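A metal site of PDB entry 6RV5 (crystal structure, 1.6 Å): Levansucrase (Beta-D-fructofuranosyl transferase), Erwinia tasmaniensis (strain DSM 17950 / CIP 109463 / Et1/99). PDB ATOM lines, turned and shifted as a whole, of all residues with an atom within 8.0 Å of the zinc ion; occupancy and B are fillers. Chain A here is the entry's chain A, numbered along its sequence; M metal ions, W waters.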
ATOM      1  N   ARG A  48       6.704  14.352   7.625  1.00  0.00           N
ATOM      2  CA  ARG A  48       7.272  13.644   6.488  1.00  0.00           C
ATOM      3  C   ARG A  48       8.157  12.454   6.932  1.00  0.00           C
ATOM      4  O   ARG A  48       8.470  12.337   8.116  1.00  0.00           O
ATOM      5  CB  ARG A  48       7.904  14.690   5.570  1.00  0.00           C
ATOM      6  CG  ARG A  48       9.217  15.294   6.034  1.00  0.00           C
ATOM      7  CD  ARG A  48       9.805  15.927   4.772  1.00  0.00           C
ATOM      8  NE  ARG A  48      11.107  16.581   4.908  1.00  0.00           N
ATOM      9  CZ  ARG A  48      12.313  16.060   4.636  1.00  0.00           C
ATOM     10  NH1 ARG A  48      12.453  14.805   4.215  1.00  0.00           N
ATOM     11  NH2 ARG A  48      13.397  16.818   4.807  1.00  0.00           N
ATOM     12  N   ASP A  49       8.491  11.578   5.955  1.00  0.00           N
ATOM     13  CA  ASP A  49       9.430  10.479   6.198  1.00  0.00           C
ATOM     14  C   ASP A  49      10.808  10.930   5.722  1.00  0.00           C
ATOM     15  O   ASP A  49      11.014  12.052   5.248  1.00  0.00           O
ATOM     16  CB  ASP A  49       8.897   9.164   5.628  1.00  0.00           C
ATOM     17  CG  ASP A  49       8.877   9.083   4.126  1.00  0.00           C
ATOM     18  OD1 ASP A  49       9.406  10.019   3.464  1.00  0.00           O
ATOM     19  OD2 ASP A  49       8.214   8.144   3.668  1.00  0.00           O
ATOM     20  N   PHE A  50      11.778  10.054   5.857  1.00  0.00           N
ATOM     21  CA  PHE A  50      13.161  10.376   5.494  1.00  0.00           C
ATOM     22  C   PHE A  50      13.351  10.521   3.967  1.00  0.00           C
ATOM     23  O   PHE A  50      14.431  10.986   3.644  1.00  0.00           O
ATOM     24  CB  PHE A  50      14.108   9.331   6.123  1.00  0.00           C
ATOM     25  CG  PHE A  50      14.536   9.628   7.539  1.00  0.00           C
ATOM     26  CD1 PHE A  50      15.220  10.802   7.861  1.00  0.00           C
ATOM     27  CD2 PHE A  50      14.307   8.729   8.557  1.00  0.00           C
ATOM     28  CE1 PHE A  50      15.607  11.073   9.165  1.00  0.00           C
ATOM     29  CE2 PHE A  50      14.730   8.978   9.843  1.00  0.00           C
ATOM     30  CZ  PHE A  50      15.389  10.143  10.144  1.00  0.00           C
ATOM     31  N   ASP A  51      12.349  10.319   3.117  1.00  0.00           N
ATOM     32  CA  ASP A  51      12.588  10.632   1.696  1.00  0.00           C
ATOM     33  C   ASP A  51      11.843  11.898   1.273  1.00  0.00           C
ATOM     34  O   ASP A  51      12.098  12.381   0.184  1.00  0.00           O
ATOM     35  CB  ASP A  51      12.354   9.434   0.782  1.00  0.00           C
ATOM     36  CG  ASP A  51      10.949   8.939   0.935  1.00  0.00           C
ATOM     37  OD1 ASP A  51      10.116   9.698   0.567  1.00  0.00           O
ATOM     38  OD2 ASP A  51      10.735   7.828   1.423  1.00  0.00           O
ATOM     39  N   GLY A  52      10.985  12.461   2.112  1.00  0.00           N
ATOM     40  CA  GLY A  52      10.340  13.715   1.712  1.00  0.00           C
ATOM     41  C   GLY A  52       8.863  13.508   1.517  1.00  0.00           C
ATOM     42  O   GLY A  52       8.155  14.482   1.507  1.00  0.00           O
ATOM     43  N   ASP A  53       8.438  12.245   1.431  1.00  0.00           N
ATOM     44  CA  ASP A  53       6.989  11.963   1.346  1.00  0.00           C
ATOM     45  C   ASP A  53       6.275  12.556   2.556  1.00  0.00           C
ATOM     46  O   ASP A  53       6.736  12.403   3.644  1.00  0.00           O
ATOM     47  CB  ASP A  53       6.681  10.480   1.488  1.00  0.00           C
ATOM     48  CG  ASP A  53       6.923   9.653   0.248  1.00  0.00           C
ATOM     49  OD1 ASP A  53       7.081  10.245  -0.813  1.00  0.00           O
ATOM     50  OD2 ASP A  53       7.068   8.451   0.416  1.00  0.00           O
ATOM     51  N   ILE A  54       5.159  13.192   2.287  1.00  0.00           N
ATOM     52  CA  ILE A  54       4.256  13.689   3.341  1.00  0.00           C
ATOM     53  C   ILE A  54       3.439  12.477   3.832  1.00  0.00           C
ATOM     54  O   ILE A  54       2.825  11.754   3.024  1.00  0.00           O
ATOM     55  CB  ILE A  54       3.356  14.793   2.831  1.00  0.00           C
ATOM     56  CG1 ILE A  54       4.159  15.885   2.095  1.00  0.00           C
ATOM     57  CG2 ILE A  54       2.518  15.366   3.987  1.00  0.00           C
ATOM     58  CD1 ILE A  54       5.403  16.402   2.817  1.00  0.00           C
ATOM     59  N   VAL A  55       3.426  12.248   5.138  1.00  0.00           N
ATOM     60  CA  VAL A  55       2.774  11.070   5.721  1.00  0.00           C
ATOM     61  C   VAL A  55       1.708  11.499   6.736  1.00  0.00           C
ATOM     62  O   VAL A  55       1.952  12.424   7.532  1.00  0.00           O
ATOM     63  CB  VAL A  55       3.798  10.133   6.394  1.00  0.00           C
ATOM     64  CG1 VAL A  55       4.707   9.496   5.378  1.00  0.00           C
ATOM     65  CG2 VAL A  55       4.588  10.827   7.497  1.00  0.00           C
ATOM     66  N   LYS A 207      19.380   7.022  -0.577  1.00  0.00           N
ATOM     67  CA  LYS A 207      19.483   5.551  -0.789  1.00  0.00           C
ATOM     68  C   LYS A 207      20.743   5.168  -1.582  1.00  0.00           C
ATOM     69  O   LYS A 207      21.160   3.998  -1.493  1.00  0.00           O
ATOM     70  CB  LYS A 207      18.224   5.023  -1.472  1.00  0.00           C
ATOM     71  CG  LYS A 207      16.985   5.037  -0.584  1.00  0.00           C
ATOM     72  CD  LYS A 207      15.777   4.436  -1.211  1.00  0.00           C
ATOM     73  CE  LYS A 207      14.497   4.808  -0.502  1.00  0.00           C
ATOM     74  NZ  LYS A 207      14.446   4.301   0.894  1.00  0.00           N
ATOM     75  N   MET A 406       0.770  12.019   1.194  1.00  0.00           N
ATOM     76  CA  MET A 406       1.064  11.154   0.038  1.00  0.00           C
ATOM     77  C   MET A 406       0.896   9.694   0.388  1.00  0.00           C
ATOM     78  O   MET A 406       0.538   8.898  -0.524  1.00  0.00           O
ATOM     79  CB  MET A 406       2.502  11.398  -0.415  1.00  0.00           C
ATOM     80  CG  MET A 406       2.651  12.819  -0.992  1.00  0.00           C
ATOM     81  SD  MET A 406       4.323  13.314  -1.243  1.00  0.00           S
ATOM     82  CE  MET A 406       4.723  12.052  -2.468  1.00  0.00           C
ATOM     83  N   LYS A 407       1.204   9.347   1.631  1.00  0.00           N
ATOM     84  CA  LYS A 407       0.852   7.992   2.103  1.00  0.00           C
ATOM     85  C   LYS A 407       0.531   8.002   3.579  1.00  0.00           C
ATOM     86  O   LYS A 407       0.863   8.962   4.315  1.00  0.00           O
ATOM     87  CB  LYS A 407       1.924   6.962   1.755  1.00  0.00           C
ATOM     88  CG  LYS A 407       3.263   7.113   2.447  1.00  0.00           C
ATOM     89  CD  LYS A 407       3.806   5.746   2.820  1.00  0.00           C
ATOM     90  CE  LYS A 407       5.256   5.581   2.433  1.00  0.00           C
ATOM     91  NZ  LYS A 407       6.013   4.866   3.461  1.00  0.00           N
ATOM     92  N   ILE A 409       0.450   6.007   7.138  1.00  0.00           N
ATOM     93  CA  ILE A 409       1.179   5.022   7.969  1.00  0.00           C
ATOM     94  C   ILE A 409       0.210   4.484   9.033  1.00  0.00           C
ATOM     95  O   ILE A 409      -0.359   5.309   9.824  1.00  0.00           O
ATOM     96  CB  ILE A 409       2.410   5.658   8.583  1.00  0.00           C
ATOM     97  CG1 ILE A 409       3.267   6.273   7.481  1.00  0.00           C
ATOM     98  CG2 ILE A 409       3.156   4.639   9.448  1.00  0.00           C
ATOM     99  CD1 ILE A 409       3.845   5.282   6.479  1.00  0.00           C
HETATM  100 ZN    ZN M   1       8.619   7.665   1.783  1.00  0.00          ZN
HETATM  101  O   HOH W   1       8.299   5.619   1.709  1.00  0.00           O
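The zinc ion is bound by the side-chain carboxylate (OD2) of Asp 49, at 2.0 Å.
Water W1 binds the zinc ion (2.1 Å).
The zinc ion is bound by OD2 of Asp 51, 2.2 Å away.
OD2 of Asp 53 binds the zinc ion, at 2.2 Å.
The zinc ion has four donor atoms within binding distance.
Slightly farther from the zinc ion lies OD1 of Asp 51 (2.8 Å).
The side-chain amino group of Lys 407 sits close to the side-chain carboxylate of Asp 49, 3.95 Å away.
OD1 of Asp 49 lies within hydrogen-bond range of N of Gly 52.
The nearest printed residue that does not touch the zinc ion is Lys 407 (4.01 Å).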
